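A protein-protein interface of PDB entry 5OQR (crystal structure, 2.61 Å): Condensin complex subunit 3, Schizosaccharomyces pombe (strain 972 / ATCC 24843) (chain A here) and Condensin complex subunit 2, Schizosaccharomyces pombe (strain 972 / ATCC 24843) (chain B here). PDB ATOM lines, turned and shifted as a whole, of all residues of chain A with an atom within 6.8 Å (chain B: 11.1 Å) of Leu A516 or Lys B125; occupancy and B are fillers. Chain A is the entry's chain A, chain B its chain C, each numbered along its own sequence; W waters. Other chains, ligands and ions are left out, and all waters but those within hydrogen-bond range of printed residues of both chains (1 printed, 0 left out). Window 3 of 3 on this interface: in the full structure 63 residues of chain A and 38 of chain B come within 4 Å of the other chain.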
ATOM      1  N   GLU A 416      -3.280 -33.741  10.600  1.00  0.00           N
ATOM      2  CA  GLU A 416      -4.590 -33.932   9.988  1.00  0.00           C
ATOM      3  C   GLU A 416      -4.498 -34.764   8.720  1.00  0.00           C
ATOM      4  O   GLU A 416      -5.417 -35.530   8.413  1.00  0.00           O
ATOM      5  CB  GLU A 416      -5.234 -32.582   9.674  1.00  0.00           C
ATOM      6  CG  GLU A 416      -5.702 -31.807  10.888  1.00  0.00           C
ATOM      7  CD  GLU A 416      -6.569 -30.622  10.512  1.00  0.00           C
ATOM      8  OE1 GLU A 416      -6.776 -30.401   9.300  1.00  0.00           O
ATOM      9  OE2 GLU A 416      -7.045 -29.915  11.425  1.00  0.00           O
ATOM     10  N   LEU A 469     -15.026 -37.688  10.631  1.00  0.00           N
ATOM     11  CA  LEU A 469     -13.803 -37.255   9.966  1.00  0.00           C
ATOM     12  C   LEU A 469     -13.762 -35.737   9.850  1.00  0.00           C
ATOM     13  O   LEU A 469     -12.815 -35.088  10.305  1.00  0.00           O
ATOM     14  CB  LEU A 469     -13.701 -37.912   8.588  1.00  0.00           C
ATOM     15  CG  LEU A 469     -12.671 -37.327   7.616  1.00  0.00           C
ATOM     16  CD1 LEU A 469     -11.279 -37.337   8.208  1.00  0.00           C
ATOM     17  CD2 LEU A 469     -12.690 -38.086   6.303  1.00  0.00           C
ATOM     18  N   PHE A 470     -14.793 -35.152   9.245  1.00  0.00           N
ATOM     19  CA  PHE A 470     -14.843 -33.711   9.049  1.00  0.00           C
ATOM     20  C   PHE A 470     -15.167 -32.950  10.326  1.00  0.00           C
ATOM     21  O   PHE A 470     -15.068 -31.719  10.334  1.00  0.00           O
ATOM     22  CB  PHE A 470     -15.860 -33.379   7.959  1.00  0.00           C
ATOM     23  CG  PHE A 470     -15.474 -33.904   6.608  1.00  0.00           C
ATOM     24  CD1 PHE A 470     -14.407 -33.355   5.922  1.00  0.00           C
ATOM     25  CD2 PHE A 470     -16.162 -34.956   6.031  1.00  0.00           C
ATOM     26  CE1 PHE A 470     -14.040 -33.837   4.687  1.00  0.00           C
ATOM     27  CE2 PHE A 470     -15.799 -35.439   4.793  1.00  0.00           C
ATOM     28  CZ  PHE A 470     -14.736 -34.878   4.121  1.00  0.00           C
ATOM     29  N   GLU A 471     -15.541 -33.644  11.399  1.00  0.00           N
ATOM     30  CA  GLU A 471     -15.669 -33.007  12.702  1.00  0.00           C
ATOM     31  C   GLU A 471     -14.324 -32.758  13.364  1.00  0.00           C
ATOM     32  O   GLU A 471     -14.244 -31.924  14.271  1.00  0.00           O
ATOM     33  CB  GLU A 471     -16.526 -33.870  13.631  1.00  0.00           C
ATOM     34  CG  GLU A 471     -17.963 -33.412  13.765  1.00  0.00           C
ATOM     35  CD  GLU A 471     -18.820 -34.403  14.528  1.00  0.00           C
ATOM     36  OE1 GLU A 471     -18.250 -35.295  15.193  1.00  0.00           O
ATOM     37  OE2 GLU A 471     -20.063 -34.297  14.460  1.00  0.00           O
ATOM     38  N   ASN A 472     -13.271 -33.452  12.932  1.00  0.00           N
ATOM     39  CA  ASN A 472     -11.983 -33.432  13.614  1.00  0.00           C
ATOM     40  C   ASN A 472     -10.881 -32.768  12.799  1.00  0.00           C
ATOM     41  O   ASN A 472      -9.704 -32.901  13.149  1.00  0.00           O
ATOM     42  CB  ASN A 472     -11.569 -34.856  13.984  1.00  0.00           C
ATOM     43  CG  ASN A 472     -12.248 -35.350  15.240  1.00  0.00           C
ATOM     44  OD1 ASN A 472     -13.274 -36.021  15.181  1.00  0.00           O
ATOM     45  ND2 ASN A 472     -11.678 -35.012  16.389  1.00  0.00           N
ATOM     46  N   ILE A 473     -11.224 -32.057  11.726  1.00  0.00           N
ATOM     47  CA  ILE A 473     -10.255 -31.270  10.979  1.00  0.00           C
ATOM     48  C   ILE A 473     -10.764 -29.838  10.896  1.00  0.00           C
ATOM     49  O   ILE A 473     -11.959 -29.568  11.030  1.00  0.00           O
ATOM     50  CB  ILE A 473      -9.984 -31.842   9.571  1.00  0.00           C
ATOM     51  CG1 ILE A 473     -11.287 -32.010   8.792  1.00  0.00           C
ATOM     52  CG2 ILE A 473      -9.263 -33.171   9.681  1.00  0.00           C
ATOM     53  CD1 ILE A 473     -11.076 -32.242   7.319  1.00  0.00           C
ATOM     54  N   THR A 474      -9.828 -28.913  10.679  1.00  0.00           N
ATOM     55  CA  THR A 474     -10.116 -27.490  10.763  1.00  0.00           C
ATOM     56  C   THR A 474      -9.894 -26.719   9.470  1.00  0.00           C
ATOM     57  O   THR A 474     -10.447 -25.623   9.332  1.00  0.00           O
ATOM     58  CB  THR A 474      -9.264 -26.841  11.865  1.00  0.00           C
ATOM     59  OG1 THR A 474      -7.909 -27.289  11.751  1.00  0.00           O
ATOM     60  CG2 THR A 474      -9.809 -27.200  13.238  1.00  0.00           C
ATOM     61  N   SER A 475      -9.109 -27.241   8.530  1.00  0.00           N
ATOM     62  CA  SER A 475      -8.856 -26.549   7.276  1.00  0.00           C
ATOM     63  C   SER A 475      -8.834 -27.558   6.140  1.00  0.00           C
ATOM     64  O   SER A 475      -8.621 -28.755   6.348  1.00  0.00           O
ATOM     65  CB  SER A 475      -7.537 -25.768   7.312  1.00  0.00           C
ATOM     66  OG  SER A 475      -6.441 -26.631   7.554  1.00  0.00           O
ATOM     67  N   SER A 476      -9.066 -27.059   4.929  1.00  0.00           N
ATOM     68  CA  SER A 476      -9.131 -27.902   3.745  1.00  0.00           C
ATOM     69  C   SER A 476      -7.790 -28.042   3.044  1.00  0.00           C
ATOM     70  O   SER A 476      -7.728 -28.629   1.959  1.00  0.00           O
ATOM     71  CB  SER A 476     -10.170 -27.348   2.764  1.00  0.00           C
ATOM     72  OG  SER A 476      -9.795 -26.069   2.287  1.00  0.00           O
ATOM     73  N   LEU A 477      -6.720 -27.527   3.636  1.00  0.00           N
ATOM     74  CA  LEU A 477      -5.416 -27.580   2.996  1.00  0.00           C
ATOM     75  C   LEU A 477      -4.909 -29.017   2.944  1.00  0.00           C
ATOM     76  O   LEU A 477      -4.962 -29.742   3.941  1.00  0.00           O
ATOM     77  CB  LEU A 477      -4.429 -26.693   3.751  1.00  0.00           C
ATOM     78  CG  LEU A 477      -3.023 -26.601   3.160  1.00  0.00           C
ATOM     79  CD1 LEU A 477      -3.054 -25.969   1.776  1.00  0.00           C
ATOM     80  CD2 LEU A 477      -2.111 -25.821   4.092  1.00  0.00           C
ATOM     81  N   GLU A 479      -6.015 -31.675   1.570  1.00  0.00           N
ATOM     82  CA  GLU A 479      -6.970 -32.778   1.593  1.00  0.00           C
ATOM     83  C   GLU A 479      -8.074 -32.601   0.557  1.00  0.00           C
ATOM     84  O   GLU A 479      -9.157 -33.174   0.711  1.00  0.00           O
ATOM     85  CB  GLU A 479      -7.576 -32.936   2.987  1.00  0.00           C
ATOM     86  CG  GLU A 479      -6.590 -33.445   4.024  1.00  0.00           C
ATOM     87  CD  GLU A 479      -6.483 -32.531   5.228  1.00  0.00           C
ATOM     88  OE1 GLU A 479      -5.383 -32.438   5.810  1.00  0.00           O
ATOM     89  OE2 GLU A 479      -7.497 -31.901   5.588  1.00  0.00           O
ATOM     90  N   MET A 483     -11.487 -35.034   0.157  1.00  0.00           N
ATOM     91  CA  MET A 483     -12.835 -34.477   0.133  1.00  0.00           C
ATOM     92  C   MET A 483     -13.576 -34.869  -1.135  1.00  0.00           C
ATOM     93  O   MET A 483     -14.690 -35.399  -1.074  1.00  0.00           O
ATOM     94  CB  MET A 483     -12.775 -32.959   0.250  1.00  0.00           C
ATOM     95  CG  MET A 483     -12.293 -32.494   1.585  1.00  0.00           C
ATOM     96  SD  MET A 483     -11.802 -30.774   1.583  1.00  0.00           S
ATOM     97  CE  MET A 483     -11.323 -30.654   3.289  1.00  0.00           C
ATOM     98  N   SER A 511     -22.851 -30.754   5.230  1.00  0.00           N
ATOM     99  CA  SER A 511     -22.718 -29.507   5.973  1.00  0.00           C
ATOM    100  C   SER A 511     -21.304 -29.338   6.507  1.00  0.00           C
ATOM    101  O   SER A 511     -20.707 -28.263   6.387  1.00  0.00           O
ATOM    102  CB  SER A 511     -23.732 -29.470   7.117  1.00  0.00           C
ATOM    103  OG  SER A 511     -25.056 -29.569   6.631  1.00  0.00           O
ATOM    104  N   LEU A 512     -20.749 -30.396   7.103  1.00  0.00           N
ATOM    105  CA  LEU A 512     -19.425 -30.299   7.709  1.00  0.00           C
ATOM    106  C   LEU A 512     -18.342 -30.058   6.669  1.00  0.00           C
ATOM    107  O   LEU A 512     -17.296 -29.487   6.991  1.00  0.00           O
ATOM    108  CB  LEU A 512     -19.119 -31.568   8.502  1.00  0.00           C
ATOM    109  CG  LEU A 512     -19.947 -31.771   9.771  1.00  0.00           C
ATOM    110  CD1 LEU A 512     -19.777 -33.180  10.295  1.00  0.00           C
ATOM    111  CD2 LEU A 512     -19.552 -30.759  10.832  1.00  0.00           C
ATOM    112  N   VAL A 513     -18.564 -30.487   5.427  1.00  0.00           N
ATOM    113  CA  VAL A 513     -17.599 -30.198   4.373  1.00  0.00           C
ATOM    114  C   VAL A 513     -17.711 -28.745   3.946  1.00  0.00           C
ATOM    115  O   VAL A 513     -16.711 -28.119   3.575  1.00  0.00           O
ATOM    116  CB  VAL A 513     -17.804 -31.154   3.183  1.00  0.00           C
ATOM    117  CG1 VAL A 513     -16.817 -30.847   2.068  1.00  0.00           C
ATOM    118  CG2 VAL A 513     -17.647 -32.590   3.632  1.00  0.00           C
ATOM    119  N   CYS A 514     -18.919 -28.183   3.992  1.00  0.00           N
ATOM    120  CA  CYS A 514     -19.098 -26.778   3.653  1.00  0.00           C
ATOM    121  C   CYS A 514     -18.382 -25.870   4.640  1.00  0.00           C
ATOM    122  O   CYS A 514     -17.963 -24.768   4.275  1.00  0.00           O
ATOM    123  CB  CYS A 514     -20.586 -26.446   3.602  1.00  0.00           C
ATOM    124  SG  CYS A 514     -21.436 -27.180   2.201  1.00  0.00           S
ATOM    125  N   LEU A 515     -18.222 -26.312   5.888  1.00  0.00           N
ATOM    126  CA  LEU A 515     -17.483 -25.534   6.874  1.00  0.00           C
ATOM    127  C   LEU A 515     -15.987 -25.501   6.598  1.00  0.00           C
ATOM    128  O   LEU A 515     -15.262 -24.790   7.301  1.00  0.00           O
ATOM    129  CB  LEU A 515     -17.728 -26.095   8.273  1.00  0.00           C
ATOM    130  CG  LEU A 515     -19.193 -26.278   8.670  1.00  0.00           C
ATOM    131  CD1 LEU A 515     -19.291 -26.824  10.084  1.00  0.00           C
ATOM    132  CD2 LEU A 515     -19.963 -24.972   8.544  1.00  0.00           C
ATOM    133  N   LEU A 516     -15.507 -26.252   5.606  1.00  0.00           N
ATOM    134  CA  LEU A 516     -14.092 -26.270   5.264  1.00  0.00           C
ATOM    135  C   LEU A 516     -13.774 -25.504   3.988  1.00  0.00           C
ATOM    136  O   LEU A 516     -12.607 -25.177   3.757  1.00  0.00           O
ATOM    137  CB  LEU A 516     -13.607 -27.717   5.115  1.00  0.00           C
ATOM    138  CG  LEU A 516     -13.745 -28.582   6.370  1.00  0.00           C
ATOM    139  CD1 LEU A 516     -13.413 -30.026   6.067  1.00  0.00           C
ATOM    140  CD2 LEU A 516     -12.852 -28.064   7.479  1.00  0.00           C
ATOM    141  N   ASN A 517     -14.775 -25.212   3.162  1.00  0.00           N
ATOM    142  CA  ASN A 517     -14.566 -24.474   1.922  1.00  0.00           C
ATOM    143  C   ASN A 517     -15.691 -23.464   1.759  1.00  0.00           C
ATOM    144  O   ASN A 517     -16.864 -23.843   1.711  1.00  0.00           O
ATOM    145  CB  ASN A 517     -14.511 -25.417   0.720  1.00  0.00           C
ATOM    146  CG  ASN A 517     -13.831 -24.791  -0.475  1.00  0.00           C
ATOM    147  OD1 ASN A 517     -14.484 -24.385  -1.434  1.00  0.00           O
ATOM    148  ND2 ASN A 517     -12.508 -24.695  -0.415  1.00  0.00           N
ATOM    149  N   ALA A 518     -15.328 -22.183   1.667  1.00  0.00           N
ATOM    150  CA  ALA A 518     -16.332 -21.128   1.586  1.00  0.00           C
ATOM    151  C   ALA A 518     -17.081 -21.170   0.261  1.00  0.00           C
ATOM    152  O   ALA A 518     -18.299 -20.960   0.224  1.00  0.00           O
ATOM    153  CB  ALA A 518     -15.672 -19.765   1.785  1.00  0.00           C
ATOM    154  N   LEU A 520     -17.668 -23.783  -1.601  1.00  0.00           N
ATOM    155  CA  LEU A 520     -18.602 -24.901  -1.555  1.00  0.00           C
ATOM    156  C   LEU A 520     -19.783 -24.583  -0.649  1.00  0.00           C
ATOM    157  O   LEU A 520     -20.927 -24.930  -0.965  1.00  0.00           O
ATOM    158  CB  LEU A 520     -17.885 -26.163  -1.078  1.00  0.00           C
ATOM    159  CG  LEU A 520     -18.706 -27.455  -1.096  1.00  0.00           C
ATOM    160  CD1 LEU A 520     -19.099 -27.835  -2.514  1.00  0.00           C
ATOM    161  CD2 LEU A 520     -17.930 -28.576  -0.442  1.00  0.00           C
ATOM    162  N   ALA A 521     -19.526 -23.925   0.481  1.00  0.00           N
ATOM    163  CA  ALA A 521     -20.613 -23.448   1.328  1.00  0.00           C
ATOM    164  C   ALA A 521     -21.570 -22.568   0.537  1.00  0.00           C
ATOM    165  O   ALA A 521     -22.787 -22.773   0.561  1.00  0.00           O
ATOM    166  CB  ALA A 521     -20.042 -22.685   2.522  1.00  0.00           C
ATOM    167  N   ASP A 549     -23.780 -21.937  10.926  1.00  0.00           N
ATOM    168  CA  ASP A 549     -22.362 -22.248  11.065  1.00  0.00           C
ATOM    169  C   ASP A 549     -21.557 -21.765   9.867  1.00  0.00           C
ATOM    170  O   ASP A 549     -20.398 -21.371  10.024  1.00  0.00           O
ATOM    171  CB  ASP A 549     -22.178 -23.749  11.267  1.00  0.00           C
ATOM    172  CG  ASP A 549     -22.475 -24.183  12.689  1.00  0.00           C
ATOM    173  OD1 ASP A 549     -23.049 -23.376  13.451  1.00  0.00           O
ATOM    174  OD2 ASP A 549     -22.138 -25.330  13.047  1.00  0.00           O
ATOM    175  N   GLN A 553     -18.462 -19.427  10.504  1.00  0.00           N
ATOM    176  CA  GLN A 553     -17.174 -19.944  10.054  1.00  0.00           C
ATOM    177  C   GLN A 553     -16.598 -19.088   8.934  1.00  0.00           C
ATOM    178  O   GLN A 553     -15.466 -18.602   9.032  1.00  0.00           O
ATOM    179  CB  GLN A 553     -17.328 -21.396   9.598  1.00  0.00           C
ATOM    180  CG  GLN A 553     -16.071 -22.021   9.002  1.00  0.00           C
ATOM    181  CD  GLN A 553     -14.959 -22.187  10.017  1.00  0.00           C
ATOM    182  OE1 GLN A 553     -15.211 -22.409  11.199  1.00  0.00           O
ATOM    183  NE2 GLN A 553     -13.719 -22.078   9.559  1.00  0.00           N
ATOM    184  N   HIS A 554     -17.362 -18.890   7.862  1.00  0.00           N
ATOM    185  CA  HIS A 554     -16.831 -18.286   6.648  1.00  0.00           C
ATOM    186  C   HIS A 554     -16.978 -16.773   6.602  1.00  0.00           C
ATOM    187  O   HIS A 554     -16.290 -16.127   5.804  1.00  0.00           O
ATOM    188  CB  HIS A 554     -17.516 -18.894   5.421  1.00  0.00           C
ATOM    189  CG  HIS A 554     -17.228 -20.349   5.237  1.00  0.00           C
ATOM    190  ND1 HIS A 554     -15.978 -20.889   5.449  1.00  0.00           N
ATOM    191  CD2 HIS A 554     -18.027 -21.380   4.880  1.00  0.00           C
ATOM    192  CE1 HIS A 554     -16.018 -22.187   5.220  1.00  0.00           C
ATOM    193  NE2 HIS A 554     -17.250 -22.510   4.872  1.00  0.00           N
ATOM    194  N   LYS B 117     -21.161 -22.178  27.420  1.00  0.00           N
ATOM    195  CA  LYS B 117     -20.154 -22.427  26.397  1.00  0.00           C
ATOM    196  C   LYS B 117     -20.768 -22.679  25.027  1.00  0.00           C
ATOM    197  O   LYS B 117     -20.072 -22.539  24.016  1.00  0.00           O
ATOM    198  CB  LYS B 117     -19.290 -23.624  26.797  1.00  0.00           C
ATOM    199  CG  LYS B 117     -18.328 -23.351  27.943  1.00  0.00           C
ATOM    200  CD  LYS B 117     -17.501 -24.584  28.277  1.00  0.00           C
ATOM    201  CE  LYS B 117     -18.316 -25.628  29.028  1.00  0.00           C
ATOM    202  NZ  LYS B 117     -17.618 -26.940  29.096  1.00  0.00           N
ATOM    203  N   ARG B 118     -22.048 -23.053  24.966  1.00  0.00           N
ATOM    204  CA  ARG B 118     -22.658 -23.380  23.682  1.00  0.00           C
ATOM    205  C   ARG B 118     -22.689 -22.184  22.745  1.00  0.00           C
ATOM    206  O   ARG B 118     -22.571 -22.350  21.526  1.00  0.00           O
ATOM    207  CB  ARG B 118     -24.081 -23.894  23.882  1.00  0.00           C
ATOM    208  CG  ARG B 118     -24.185 -25.188  24.654  1.00  0.00           C
ATOM    209  CD  ARG B 118     -25.607 -25.710  24.610  1.00  0.00           C
ATOM    210  NE  ARG B 118     -26.013 -26.018  23.243  1.00  0.00           N
ATOM    211  CZ  ARG B 118     -27.255 -26.316  22.873  1.00  0.00           C
ATOM    212  NH1 ARG B 118     -28.232 -26.346  23.768  1.00  0.00           N
ATOM    213  NH2 ARG B 118     -27.516 -26.580  21.600  1.00  0.00           N
ATOM    214  N   LEU B 119     -22.861 -20.979  23.289  1.00  0.00           N
ATOM    215  CA  LEU B 119     -23.124 -19.814  22.450  1.00  0.00           C
ATOM    216  C   LEU B 119     -22.012 -19.604  21.431  1.00  0.00           C
ATOM    217  O   LEU B 119     -22.277 -19.390  20.243  1.00  0.00           O
ATOM    218  CB  LEU B 119     -23.292 -18.573  23.325  1.00  0.00           C
ATOM    219  CG  LEU B 119     -23.887 -17.356  22.615  1.00  0.00           C
ATOM    220  CD1 LEU B 119     -25.365 -17.574  22.326  1.00  0.00           C
ATOM    221  CD2 LEU B 119     -23.679 -16.098  23.440  1.00  0.00           C
ATOM    222  N   LEU B 120     -20.763 -19.655  21.875  1.00  0.00           N
ATOM    223  CA  LEU B 120     -19.625 -19.407  21.004  1.00  0.00           C
ATOM    224  C   LEU B 120     -19.095 -20.675  20.349  1.00  0.00           C
ATOM    225  O   LEU B 120     -18.008 -20.650  19.765  1.00  0.00           O
ATOM    226  CB  LEU B 120     -18.514 -18.712  21.793  1.00  0.00           C
ATOM    227  CG  LEU B 120     -18.953 -17.403  22.459  1.00  0.00           C
ATOM    228  CD1 LEU B 120     -17.857 -16.853  23.352  1.00  0.00           C
ATOM    229  CD2 LEU B 120     -19.359 -16.369  21.419  1.00  0.00           C
ATOM    230  N   GLN B 121     -19.834 -21.775  20.435  1.00  0.00           N
ATOM    231  CA  GLN B 121     -19.506 -23.003  19.729  1.00  0.00           C
ATOM    232  C   GLN B 121     -20.318 -23.098  18.446  1.00  0.00           C
ATOM    233  O   GLN B 121     -21.437 -22.590  18.358  1.00  0.00           O
ATOM    234  CB  GLN B 121     -19.794 -24.231  20.592  1.00  0.00           C
ATOM    235  CG  GLN B 121     -18.851 -24.432  21.756  1.00  0.00           C
ATOM    236  CD  GLN B 121     -19.300 -25.562  22.656  1.00  0.00           C
ATOM    237  OE1 GLN B 121     -20.426 -26.044  22.547  1.00  0.00           O
ATOM    238  NE2 GLN B 121     -18.422 -25.994  23.549  1.00  0.00           N
ATOM    239  N   LEU B 122     -19.743 -23.764  17.452  1.00  0.00           N
ATOM    240  CA  LEU B 122     -20.495 -24.102  16.256  1.00  0.00           C
ATOM    241  C   LEU B 122     -21.483 -25.217  16.566  1.00  0.00           C
ATOM    242  O   LEU B 122     -21.185 -26.140  17.329  1.00  0.00           O
ATOM    243  CB  LEU B 122     -19.552 -24.533  15.135  1.00  0.00           C
ATOM    244  CG  LEU B 122     -18.611 -23.467  14.578  1.00  0.00           C
ATOM    245  CD1 LEU B 122     -17.567 -24.109  13.685  1.00  0.00           C
ATOM    246  CD2 LEU B 122     -19.385 -22.410  13.809  1.00  0.00           C
ATOM    247  N   PHE B 123     -22.676 -25.121  15.980  1.00  0.00           N
ATOM    248  CA  PHE B 123     -23.683 -26.158  16.170  1.00  0.00           C
ATOM    249  C   PHE B 123     -23.126 -27.533  15.826  1.00  0.00           C
ATOM    250  O   PHE B 123     -23.304 -28.499  16.576  1.00  0.00           O
ATOM    251  CB  PHE B 123     -24.907 -25.859  15.303  1.00  0.00           C
ATOM    252  CG  PHE B 123     -25.826 -24.815  15.867  1.00  0.00           C
ATOM    253  CD1 PHE B 123     -26.301 -24.909  17.162  1.00  0.00           C
ATOM    254  CD2 PHE B 123     -26.227 -23.743  15.091  1.00  0.00           C
ATOM    255  CE1 PHE B 123     -27.152 -23.953  17.671  1.00  0.00           C
ATOM    256  CE2 PHE B 123     -27.078 -22.786  15.594  1.00  0.00           C
ATOM    257  CZ  PHE B 123     -27.541 -22.890  16.887  1.00  0.00           C
ATOM    258  N   LEU B 124     -22.443 -27.634  14.691  1.00  0.00           N
ATOM    259  CA  LEU B 124     -22.047 -28.916  14.132  1.00  0.00           C
ATOM    260  C   LEU B 124     -20.650 -29.354  14.547  1.00  0.00           C
ATOM    261  O   LEU B 124     -20.312 -30.530  14.371  1.00  0.00           O
ATOM    262  CB  LEU B 124     -22.126 -28.854  12.606  1.00  0.00           C
ATOM    263  CG  LEU B 124     -23.485 -28.430  12.046  1.00  0.00           C
ATOM    264  CD1 LEU B 124     -23.391 -28.161  10.555  1.00  0.00           C
ATOM    265  CD2 LEU B 124     -24.535 -29.486  12.336  1.00  0.00           C
ATOM    266  N   LYS B 125     -19.837 -28.454  15.091  1.00  0.00           N
ATOM    267  CA  LYS B 125     -18.476 -28.769  15.525  1.00  0.00           C
ATOM    268  C   LYS B 125     -18.268 -28.214  16.926  1.00  0.00           C
ATOM    269  O   LYS B 125     -17.523 -27.250  17.128  1.00  0.00           O
ATOM    270  CB  LYS B 125     -17.450 -28.209  14.539  1.00  0.00           C
ATOM    271  CG  LYS B 125     -17.416 -28.984  13.231  1.00  0.00           C
ATOM    272  CD  LYS B 125     -16.682 -28.253  12.119  1.00  0.00           C
ATOM    273  CE  LYS B 125     -15.177 -28.356  12.256  1.00  0.00           C
ATOM    274  NZ  LYS B 125     -14.502 -28.277  10.931  1.00  0.00           N
ATOM    275  N   PRO B 126     -18.913 -28.814  17.928  1.00  0.00           N
ATOM    276  CA  PRO B 126     -18.813 -28.261  19.289  1.00  0.00           C
ATOM    277  C   PRO B 126     -17.392 -28.179  19.818  1.00  0.00           C
ATOM    278  O   PRO B 126     -17.029 -27.178  20.450  1.00  0.00           O
ATOM    279  CB  PRO B 126     -19.665 -29.229  20.121  1.00  0.00           C
ATOM    280  CG  PRO B 126     -20.576 -29.882  19.147  1.00  0.00           C
ATOM    281  CD  PRO B 126     -19.811 -29.979  17.870  1.00  0.00           C
ATOM    282  N   LYS B 127     -16.577 -29.215  19.608  1.00  0.00           N
ATOM    283  CA  LYS B 127     -15.202 -29.232  20.096  1.00  0.00           C
ATOM    284  C   LYS B 127     -14.236 -28.488  19.179  1.00  0.00           C
ATOM    285  O   LYS B 127     -13.062 -28.877  19.077  1.00  0.00           O
ATOM    286  CB  LYS B 127     -14.739 -30.676  20.294  1.00  0.00           C
ATOM    287  CG  LYS B 127     -15.765 -31.577  20.969  1.00  0.00           C
ATOM    288  CD  LYS B 127     -15.088 -32.694  21.748  1.00  0.00           C
ATOM    289  CE  LYS B 127     -16.082 -33.746  22.209  1.00  0.00           C
ATOM    290  NZ  LYS B 127     -15.442 -34.770  23.082  1.00  0.00           N
ATOM    291  N   MET B 128     -14.687 -27.421  18.526  1.00  0.00           N
ATOM    292  CA  MET B 128     -13.862 -26.668  17.601  1.00  0.00           C
ATOM    293  C   MET B 128     -12.651 -26.082  18.318  1.00  0.00           C
ATOM    294  O   MET B 128     -12.635 -25.968  19.546  1.00  0.00           O
ATOM    295  CB  MET B 128     -14.683 -25.555  16.953  1.00  0.00           C
ATOM    296  CG  MET B 128     -13.976 -24.830  15.837  1.00  0.00           C
ATOM    297  SD  MET B 128     -13.483 -25.936  14.498  1.00  0.00           S
ATOM    298  CE  MET B 128     -12.922 -24.766  13.267  1.00  0.00           C
HETATM  299  O   HOH W   1     -15.676 -29.579   8.787  1.00  0.00           O
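Among the printed residues, merely in contact across the chains: Asp A549 with Leu B122, Phe A470 with Lys B125, Leu A515 with Lys B125, Leu A512 with Leu B124, Leu A512 with Lys B125, Ser A511 with Leu B124, Glu A471 with Leu B124, Gln A553 with Leu B122, Leu A516 with Lys B125, Gln A553 with Met B128 and Thr A474 with Met B128.
Water W1 lies within hydrogen-bond range of O of Leu A512, O of Phe A470 and NZ of Lys B125.
The side-chain hydroxyl (OG1) of Thr A474 lies within hydrogen-bond range of the side-chain carboxylate (OE2) of Glu A416 (2.8 Å). The side-chain hydroxyl (OG) of Ser A476 sits at hydrogen-bond distance from the backbone carbonyl oxygen (O) of Leu A516 (3.3 Å).
The backbone NH (N) of Leu B124 sits at hydrogen-bond distance from the side-chain carboxylate (OD2) of Asp A549 (2.8 Å). The side-chain carboxylate (OD2) of Asp A549 is in hydrogen-bond range of the backbone NH (N) of Phe B123 (3.0 Å). O of Ile A473 sits at hydrogen-bond distance from NZ of Lys B125 (2.9 Å).
Of chain B, only Lys B125 (3.8 Å) comes within 4 Å of Leu A516. Of the printed residues of chain A, Lys B125 touches Phe A470, Ile A473, Leu A512, Leu A515 and Leu A516. Phe A470 touches one residue of chain B. Of the printed residues of chain B, Glu A471 touches Leu B124. Ile A473 touches one residue of chain B. Thr A474 touches just one residue of chain B: Met B128. No residue of chain B comes within 4 Å of Ser A475. No residue of chain B comes within 4 Å of Ser A476. Cys A514 touches none of the printed residues of chain B. Leu A515 touches just one residue of chain B: Lys B125 (3.6 Å). No residue of chain B comes within 4 Å of Asn A517. Printed residues of chain A within 4 Å of Leu B124: Glu A471, Ser A511, Leu A512 and Asp A549. Of the printed residues of chain A, Phe B123 touches Asp A549. Printed residues of chain A within 4 Å of Leu B122: Asp A549 and Gln A553. Of the printed residues of chain B, Gln A553 touches Leu B122 and Met B128. Of the printed residues of chain B, Asp A549 touches Leu B122, Phe B123 and Leu B124. Met A483 touches none of the printed residues of chain B. Asn A472 touches none of the printed residues of chain B. The nearest residue of chain A that does not touch Lys B125 is Glu A471 (4.2 Å). The nearest printed residue of chain A that does not touch Leu B124 is Leu A515 (4.3 Å).
Along chain B the printed residues that touch a printed residue of chain A span positions 122 to 128. Of the 25 printed residues of chain A, 10 touch a printed residue of chain B. Among the printed residues, no Asp or Glu carboxylate lies within 4 Å of a Lys or Arg side-chain nitrogen of the other chain.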
